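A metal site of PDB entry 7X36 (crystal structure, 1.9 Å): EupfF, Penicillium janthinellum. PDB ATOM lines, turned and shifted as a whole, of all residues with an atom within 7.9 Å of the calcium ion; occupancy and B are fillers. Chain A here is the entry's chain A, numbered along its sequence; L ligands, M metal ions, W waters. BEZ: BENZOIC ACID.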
ATOM      1  N   TRP A  48     -30.272  25.180  15.873  1.00  0.00           N
ATOM      2  CA  TRP A  48     -30.025  25.333  14.441  1.00  0.00           C
ATOM      3  C   TRP A  48     -31.018  24.438  13.711  1.00  0.00           C
ATOM      4  O   TRP A  48     -30.899  23.213  13.753  1.00  0.00           O
ATOM      5  CB  TRP A  48     -28.558  24.965  14.163  1.00  0.00           C
ATOM      6  CG  TRP A  48     -28.088  24.810  12.748  1.00  0.00           C
ATOM      7  CD1 TRP A  48     -28.846  24.573  11.618  1.00  0.00           C
ATOM      8  CD2 TRP A  48     -26.724  24.877  12.307  1.00  0.00           C
ATOM      9  NE1 TRP A  48     -28.030  24.469  10.538  1.00  0.00           N
ATOM     10  CE2 TRP A  48     -26.733  24.657  10.915  1.00  0.00           C
ATOM     11  CE3 TRP A  48     -25.503  25.091  12.955  1.00  0.00           C
ATOM     12  CZ2 TRP A  48     -25.552  24.664  10.145  1.00  0.00           C
ATOM     13  CZ3 TRP A  48     -24.329  25.086  12.195  1.00  0.00           C
ATOM     14  CH2 TRP A  48     -24.367  24.870  10.796  1.00  0.00           C
ATOM     15  N   GLU A  50     -32.264  22.982  10.375  1.00  0.00           N
ATOM     16  CA  GLU A  50     -31.494  22.766   9.157  1.00  0.00           C
ATOM     17  C   GLU A  50     -32.311  22.316   7.952  1.00  0.00           C
ATOM     18  O   GLU A  50     -31.971  22.674   6.822  1.00  0.00           O
ATOM     19  CB  GLU A  50     -30.384  21.750   9.435  1.00  0.00           C
ATOM     20  CG  GLU A  50     -29.612  21.261   8.226  1.00  0.00           C
ATOM     21  CD  GLU A  50     -28.914  22.353   7.428  1.00  0.00           C
ATOM     22  OE1 GLU A  50     -28.454  22.048   6.305  1.00  0.00           O
ATOM     23  OE2 GLU A  50     -28.807  23.513   7.900  1.00  0.00           O
ATOM     24  N   ASN A  51     -33.361  21.513   8.134  1.00  0.00           N
ATOM     25  CA  ASN A  51     -34.161  21.087   7.000  1.00  0.00           C
ATOM     26  C   ASN A  51     -35.572  20.748   7.451  1.00  0.00           C
ATOM     27  O   ASN A  51     -35.895  20.799   8.648  1.00  0.00           O
ATOM     28  CB  ASN A  51     -33.530  19.898   6.281  1.00  0.00           C
ATOM     29  CG  ASN A  51     -33.648  20.053   4.770  1.00  0.00           C
ATOM     30  OD1 ASN A  51     -34.761  20.146   4.256  1.00  0.00           O
ATOM     31  ND2 ASN A  51     -32.507  20.157   4.072  1.00  0.00           N
ATOM     32  N   SER A  65     -29.579  20.657  13.871  1.00  0.00           N
ATOM     33  CA  SER A  65     -28.162  20.307  13.886  1.00  0.00           C
ATOM     34  C   SER A  65     -27.557  20.537  15.257  1.00  0.00           C
ATOM     35  O   SER A  65     -26.705  19.753  15.702  1.00  0.00           O
ATOM     36  CB  SER A  65     -27.399  21.112  12.840  1.00  0.00           C
ATOM     37  OG  SER A  65     -27.779  20.704  11.541  1.00  0.00           O
ATOM     38  N   ILE A  98     -28.716  16.618   9.652  1.00  0.00           N
ATOM     39  CA  ILE A  98     -28.599  17.620   8.603  1.00  0.00           C
ATOM     40  C   ILE A  98     -29.873  17.554   7.750  1.00  0.00           C
ATOM     41  O   ILE A  98     -30.907  18.107   8.148  1.00  0.00           O
ATOM     42  CB  ILE A  98     -27.270  17.412   7.821  1.00  0.00           C
ATOM     43  CG1 ILE A  98     -26.140  17.302   8.855  1.00  0.00           C
ATOM     44  CG2 ILE A  98     -26.948  18.574   6.929  1.00  0.00           C
ATOM     45  CD1 ILE A  98     -24.726  17.618   8.308  1.00  0.00           C
ATOM     46  N   GLY A  99     -29.845  16.812   6.648  1.00  0.00           N
ATOM     47  CA  GLY A  99     -31.000  16.721   5.776  1.00  0.00           C
ATOM     48  C   GLY A  99     -32.026  15.658   6.188  1.00  0.00           C
ATOM     49  O   GLY A  99     -31.796  14.802   7.037  1.00  0.00           O
ATOM     50  N   LEU A 154     -19.515  14.525   3.970  1.00  0.00           N
ATOM     51  CA  LEU A 154     -20.564  15.130   4.807  1.00  0.00           C
ATOM     52  C   LEU A 154     -21.911  14.997   4.098  1.00  0.00           C
ATOM     53  O   LEU A 154     -22.141  15.644   3.061  1.00  0.00           O
ATOM     54  CB  LEU A 154     -20.226  16.584   5.137  1.00  0.00           C
ATOM     55  CG  LEU A 154     -21.328  17.400   5.822  1.00  0.00           C
ATOM     56  CD1 LEU A 154     -20.784  18.210   6.994  1.00  0.00           C
ATOM     57  CD2 LEU A 154     -22.074  18.295   4.793  1.00  0.00           C
ATOM     58  N   LEU A 155     -22.792  14.171   4.630  1.00  0.00           N
ATOM     59  CA  LEU A 155     -24.095  13.994   4.014  1.00  0.00           C
ATOM     60  C   LEU A 155     -24.966  15.208   4.280  1.00  0.00           C
ATOM     61  O   LEU A 155     -25.046  15.720   5.408  1.00  0.00           O
ATOM     62  CB  LEU A 155     -24.780  12.736   4.525  1.00  0.00           C
ATOM     63  CG  LEU A 155     -23.999  11.445   4.328  1.00  0.00           C
ATOM     64  CD1 LEU A 155     -24.790  10.277   4.945  1.00  0.00           C
ATOM     65  CD2 LEU A 155     -23.717  11.231   2.838  1.00  0.00           C
ATOM     66  N   GLN A 156     -25.651  15.675   3.231  1.00  0.00           N
ATOM     67  CA  GLN A 156     -26.309  16.964   3.250  1.00  0.00           C
ATOM     68  C   GLN A 156     -27.801  16.853   2.943  1.00  0.00           C
ATOM     69  O   GLN A 156     -28.621  16.903   3.859  1.00  0.00           O
ATOM     70  CB  GLN A 156     -25.617  17.898   2.261  1.00  0.00           C
ATOM     71  CG  GLN A 156     -26.252  19.261   2.117  1.00  0.00           C
ATOM     72  CD  GLN A 156     -26.067  20.111   3.350  1.00  0.00           C
ATOM     73  OE1 GLN A 156     -27.013  20.345   4.086  1.00  0.00           O
ATOM     74  NE2 GLN A 156     -24.845  20.575   3.577  1.00  0.00           N
ATOM     75  N   GLY A 157     -28.181  16.695   1.660  1.00  0.00           N
ATOM     76  CA  GLY A 157     -29.568  16.568   1.296  1.00  0.00           C
ATOM     77  C   GLY A 157     -29.978  15.151   0.925  1.00  0.00           C
ATOM     78  O   GLY A 157     -29.139  14.356   0.511  1.00  0.00           O
ATOM     79  N   SER A 171     -26.772  14.024  -1.136  1.00  0.00           N
ATOM     80  CA  SER A 171     -25.650  14.883  -1.496  1.00  0.00           C
ATOM     81  C   SER A 171     -24.569  14.912  -0.396  1.00  0.00           C
ATOM     82  O   SER A 171     -24.803  14.570   0.775  1.00  0.00           O
ATOM     83  CB  SER A 171     -26.160  16.279  -1.824  1.00  0.00           C
ATOM     84  OG  SER A 171     -26.699  16.885  -0.686  1.00  0.00           O
ATOM     85  N   VAL A 222     -20.127  25.104   1.611  1.00  0.00           N
ATOM     86  CA  VAL A 222     -20.166  23.856   0.857  1.00  0.00           C
ATOM     87  C   VAL A 222     -20.315  24.176  -0.622  1.00  0.00           C
ATOM     88  O   VAL A 222     -20.641  25.295  -0.996  1.00  0.00           O
ATOM     89  CB  VAL A 222     -21.300  22.921   1.308  1.00  0.00           C
ATOM     90  CG1 VAL A 222     -21.045  22.421   2.795  1.00  0.00           C
ATOM     91  CG2 VAL A 222     -22.683  23.597   1.126  1.00  0.00           C
ATOM     92  N   ILE A 224     -22.142  21.546  -3.585  1.00  0.00           N
ATOM     93  CA  ILE A 224     -23.493  21.007  -3.640  1.00  0.00           C
ATOM     94  C   ILE A 224     -24.112  21.008  -2.251  1.00  0.00           C
ATOM     95  O   ILE A 224     -23.522  20.521  -1.279  1.00  0.00           O
ATOM     96  CB  ILE A 224     -23.505  19.603  -4.260  1.00  0.00           C
ATOM     97  CG1 ILE A 224     -24.945  19.098  -4.294  1.00  0.00           C
ATOM     98  CG2 ILE A 224     -22.579  18.640  -3.431  1.00  0.00           C
ATOM     99  CD1 ILE A 224     -25.159  17.843  -5.189  1.00  0.00           C
ATOM    100  N   ASN A 225     -25.313  21.574  -2.146  1.00  0.00           N
ATOM    101  CA  ASN A 225     -26.055  21.610  -0.887  1.00  0.00           C
ATOM    102  C   ASN A 225     -27.351  20.810  -1.090  1.00  0.00           C
ATOM    103  O   ASN A 225     -27.290  19.585  -1.253  1.00  0.00           O
ATOM    104  CB  ASN A 225     -26.261  23.069  -0.452  1.00  0.00           C
ATOM    105  CG  ASN A 225     -26.459  23.221   1.069  1.00  0.00           C
ATOM    106  OD1 ASN A 225     -27.043  22.354   1.682  1.00  0.00           O
ATOM    107  ND2 ASN A 225     -25.993  24.326   1.643  1.00  0.00           N
ATOM    108  N   GLY A 226     -28.525  21.445  -1.140  1.00  0.00           N
ATOM    109  CA  GLY A 226     -29.750  20.669  -1.249  1.00  0.00           C
ATOM    110  C   GLY A 226     -29.849  19.915  -2.563  1.00  0.00           C
ATOM    111  O   GLY A 226     -29.361  20.348  -3.610  1.00  0.00           O
ATOM    112  N   ILE A 227     -30.536  18.763  -2.523  1.00  0.00           N
ATOM    113  CA  ILE A 227     -30.973  18.069  -3.735  1.00  0.00           C
ATOM    114  C   ILE A 227     -32.468  17.807  -3.635  1.00  0.00           C
ATOM    115  O   ILE A 227     -32.975  17.533  -2.554  1.00  0.00           O
ATOM    116  CB  ILE A 227     -30.224  16.729  -3.946  1.00  0.00           C
ATOM    117  CG1 ILE A 227     -30.192  15.901  -2.647  1.00  0.00           C
ATOM    118  CG2 ILE A 227     -28.803  16.988  -4.414  1.00  0.00           C
ATOM    119  CD1 ILE A 227     -29.817  14.406  -2.886  1.00  0.00           C
ATOM    120  N   VAL A 237     -28.531  22.608  -5.887  1.00  0.00           N
ATOM    121  CA  VAL A 237     -28.034  23.982  -5.819  1.00  0.00           C
ATOM    122  C   VAL A 237     -26.604  23.963  -5.336  1.00  0.00           C
ATOM    123  O   VAL A 237     -26.199  23.108  -4.520  1.00  0.00           O
ATOM    124  CB  VAL A 237     -28.907  24.866  -4.918  1.00  0.00           C
ATOM    125  CG1 VAL A 237     -30.314  25.040  -5.501  1.00  0.00           C
ATOM    126  CG2 VAL A 237     -28.970  24.316  -3.464  1.00  0.00           C
ATOM    127  N   GLN A 239     -23.901  26.181  -3.263  1.00  0.00           N
ATOM    128  CA  GLN A 239     -23.805  27.285  -2.317  1.00  0.00           C
ATOM    129  C   GLN A 239     -22.656  28.231  -2.663  1.00  0.00           C
ATOM    130  O   GLN A 239     -22.677  29.390  -2.249  1.00  0.00           O
ATOM    131  CB  GLN A 239     -23.604  26.745  -0.877  1.00  0.00           C
ATOM    132  CG  GLN A 239     -23.561  27.838   0.224  1.00  0.00           C
ATOM    133  CD  GLN A 239     -23.708  27.299   1.628  1.00  0.00           C
ATOM    134  OE1 GLN A 239     -22.788  26.672   2.160  1.00  0.00           O
ATOM    135  NE2 GLN A 239     -24.862  27.566   2.254  1.00  0.00           N
ATOM    136  N   TRP A 272     -27.012  29.623  -1.935  1.00  0.00           N
ATOM    137  CA  TRP A 272     -28.137  28.693  -1.911  1.00  0.00           C
ATOM    138  C   TRP A 272     -27.942  27.588  -0.883  1.00  0.00           C
ATOM    139  O   TRP A 272     -26.845  27.040  -0.719  1.00  0.00           O
ATOM    140  CB  TRP A 272     -28.312  28.026  -3.269  1.00  0.00           C
ATOM    141  CG  TRP A 272     -28.524  28.919  -4.490  1.00  0.00           C
ATOM    142  CD1 TRP A 272     -27.857  28.821  -5.678  1.00  0.00           C
ATOM    143  CD2 TRP A 272     -29.460  29.995  -4.645  1.00  0.00           C
ATOM    144  NE1 TRP A 272     -28.331  29.769  -6.565  1.00  0.00           N
ATOM    145  CE2 TRP A 272     -29.306  30.496  -5.957  1.00  0.00           C
ATOM    146  CE3 TRP A 272     -30.423  30.582  -3.804  1.00  0.00           C
ATOM    147  CZ2 TRP A 272     -30.079  31.555  -6.456  1.00  0.00           C
ATOM    148  CZ3 TRP A 272     -31.191  31.636  -4.295  1.00  0.00           C
ATOM    149  CH2 TRP A 272     -31.005  32.123  -5.609  1.00  0.00           C
ATOM    150  N   ASP A 273     -29.050  27.190  -0.248  1.00  0.00           N
ATOM    151  CA  ASP A 273     -29.045  26.091   0.721  1.00  0.00           C
ATOM    152  C   ASP A 273     -29.976  24.951   0.288  1.00  0.00           C
ATOM    153  O   ASP A 273     -29.471  23.903  -0.123  1.00  0.00           O
ATOM    154  CB  ASP A 273     -29.356  26.636   2.110  1.00  0.00           C
ATOM    155  CG  ASP A 273     -28.813  25.754   3.199  1.00  0.00           C
ATOM    156  OD1 ASP A 273     -28.702  24.547   2.926  1.00  0.00           O
ATOM    157  OD2 ASP A 273     -28.514  26.248   4.308  1.00  0.00           O
ATOM    158  N   ASP A 274     -31.303  25.124   0.293  1.00  0.00           N
ATOM    159  CA  ASP A 274     -32.197  24.084  -0.204  1.00  0.00           C
ATOM    160  C   ASP A 274     -33.439  24.721  -0.861  1.00  0.00           C
ATOM    161  O   ASP A 274     -33.568  25.945  -0.951  1.00  0.00           O
ATOM    162  CB  ASP A 274     -32.567  23.113   0.919  1.00  0.00           C
ATOM    163  CG  ASP A 274     -32.681  21.659   0.432  1.00  0.00           C
ATOM    164  OD1 ASP A 274     -33.303  21.457  -0.620  1.00  0.00           O
ATOM    165  OD2 ASP A 274     -32.192  20.711   1.113  1.00  0.00           O
ATOM    166  N   THR A 288     -33.796  28.901  -0.848  1.00  0.00           N
ATOM    167  CA  THR A 288     -33.241  29.778   0.162  1.00  0.00           C
ATOM    168  C   THR A 288     -31.842  30.194  -0.259  1.00  0.00           C
ATOM    169  O   THR A 288     -31.047  29.405  -0.789  1.00  0.00           O
ATOM    170  CB  THR A 288     -33.222  29.107   1.557  1.00  0.00           C
ATOM    171  OG1 THR A 288     -32.187  28.114   1.616  1.00  0.00           O
ATOM    172  CG2 THR A 288     -34.576  28.431   1.904  1.00  0.00           C
ATOM    173  N   PRO A 320     -31.963  31.585   6.376  1.00  0.00           N
ATOM    174  CA  PRO A 320     -32.868  30.472   6.025  1.00  0.00           C
ATOM    175  C   PRO A 320     -32.051  29.266   5.557  1.00  0.00           C
ATOM    176  O   PRO A 320     -30.935  29.411   5.058  1.00  0.00           O
ATOM    177  CB  PRO A 320     -33.725  31.049   4.894  1.00  0.00           C
ATOM    178  CG  PRO A 320     -32.789  32.026   4.203  1.00  0.00           C
ATOM    179  CD  PRO A 320     -31.904  32.604   5.292  1.00  0.00           C
ATOM    180  N   THR A 321     -32.611  28.066   5.755  1.00  0.00           N
ATOM    181  CA  THR A 321     -31.850  26.843   5.494  1.00  0.00           C
ATOM    182  C   THR A 321     -32.569  25.895   4.533  1.00  0.00           C
ATOM    183  O   THR A 321     -31.904  25.161   3.770  1.00  0.00           O
ATOM    184  CB  THR A 321     -31.516  26.102   6.808  1.00  0.00           C
ATOM    185  OG1 THR A 321     -32.699  25.966   7.614  1.00  0.00           O
ATOM    186  CG2 THR A 321     -30.467  26.854   7.571  1.00  0.00           C
ATOM    187  N   SER A 322     -33.896  25.882   4.538  1.00  0.00           N
ATOM    188  CA  SER A 322     -34.600  24.979   3.623  1.00  0.00           C
ATOM    189  C   SER A 322     -36.042  25.445   3.487  1.00  0.00           C
ATOM    190  O   SER A 322     -36.487  26.326   4.205  1.00  0.00           O
ATOM    191  CB  SER A 322     -34.509  23.538   4.125  1.00  0.00           C
ATOM    192  OG  SER A 322     -34.984  22.614   3.170  1.00  0.00           O
HETATM  193  C   BEZ L   1     -24.911  21.396   9.801  1.00  0.00           C
HETATM  194  O1  BEZ L   1     -26.136  21.457   9.543  1.00  0.00           O
HETATM  195  O2  BEZ L   1     -24.587  21.141  10.983  1.00  0.00           O
HETATM  196  C1  BEZ L   1     -23.873  21.656   8.721  1.00  0.00           C
HETATM  197  C2  BEZ L   1     -22.530  21.901   9.042  1.00  0.00           C
HETATM  198  C3  BEZ L   1     -21.588  22.153   8.038  1.00  0.00           C
HETATM  199  C4  BEZ L   1     -21.989  22.168   6.693  1.00  0.00           C
HETATM  200  C5  BEZ L   1     -23.328  21.945   6.371  1.00  0.00           C
HETATM  201  C6  BEZ L   1     -24.266  21.688   7.382  1.00  0.00           C
HETATM  202 CA    CA M   1     -28.342  22.251   3.912  1.00  0.00          CA
HETATM  203  O   HOH W   1     -29.792  19.817   4.903  1.00  0.00           O
HETATM  204  O   HOH W   2     -30.675  22.794   4.459  1.00  0.00           O
HETATM  205  O   HOH W   3     -26.367  23.646   4.608  1.00  0.00           O
HETATM  206  O   HOH W   4     -29.503  21.430   1.887  1.00  0.00           O
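O of Gln 156 lies within hydrogen-bond range of N of Gly 99, at 3.0 Å.
The backbone NH (N) of Gln 156 is in hydrogen-bond range of the backbone carbonyl oxygen (O) of Ser 171, at 2.8 Å.
OG1 of Thr 321 sits close to O of Glu 50, at 3.5 Å.
The side-chain carboxylate (OE2) of Glu 50 lies within hydrogen-bond range of the indole nitrogen (NE1) of Trp 48, 2.9 Å away.
The backbone carbonyl oxygen of Asp 273 sits at hydrogen-bond distance from the backbone NH of Gly 226 (2.8 Å).
The backbone NH (N) of Asp 273 sits at hydrogen-bond distance from the backbone carbonyl oxygen (O) of Thr 288 (3.0 Å).
The side-chain amide nitrogen of Asn 225 sits close to the side-chain amide nitrogen of Gln 239 (3.5 Å).
OG of Ser 171 sits at hydrogen-bond distance from O of Asn 225.
The calcium ion is bound by OE1 of Gln 156, OE1 of Glu 50, water W2, water W4, water W3, OD1 of Asp 273 and OD1 of Asn 225.
Slightly farther from the calcium ion lies water W1 (3.0 Å).
An oxygen (O1) of the ligand is in hydrogen-bond range of the side-chain hydroxyl (OG) of Ser 65, 2.7 Å away.
Water W4 lies within hydrogen-bond range of OD2 of Asp 274, N of Gly 226 and O of Asp 273.
Water W3 bridges the side-chain amide nitrogen (ND2) of Asn 225 and the side-chain carboxylate (OD2) of Asp 273.
Water W2 lies within hydrogen-bond range of the backbone carbonyl oxygen of Glu 50, the backbone carbonyl oxygen of Thr 321 and the side-chain amide nitrogen of Asn 51.
Water W1 lies within hydrogen-bond range of the side-chain amide nitrogen (ND2) of Asn 51, the backbone carbonyl oxygen (O) of Gln 156 and the backbone NH (N) of Gly 99.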
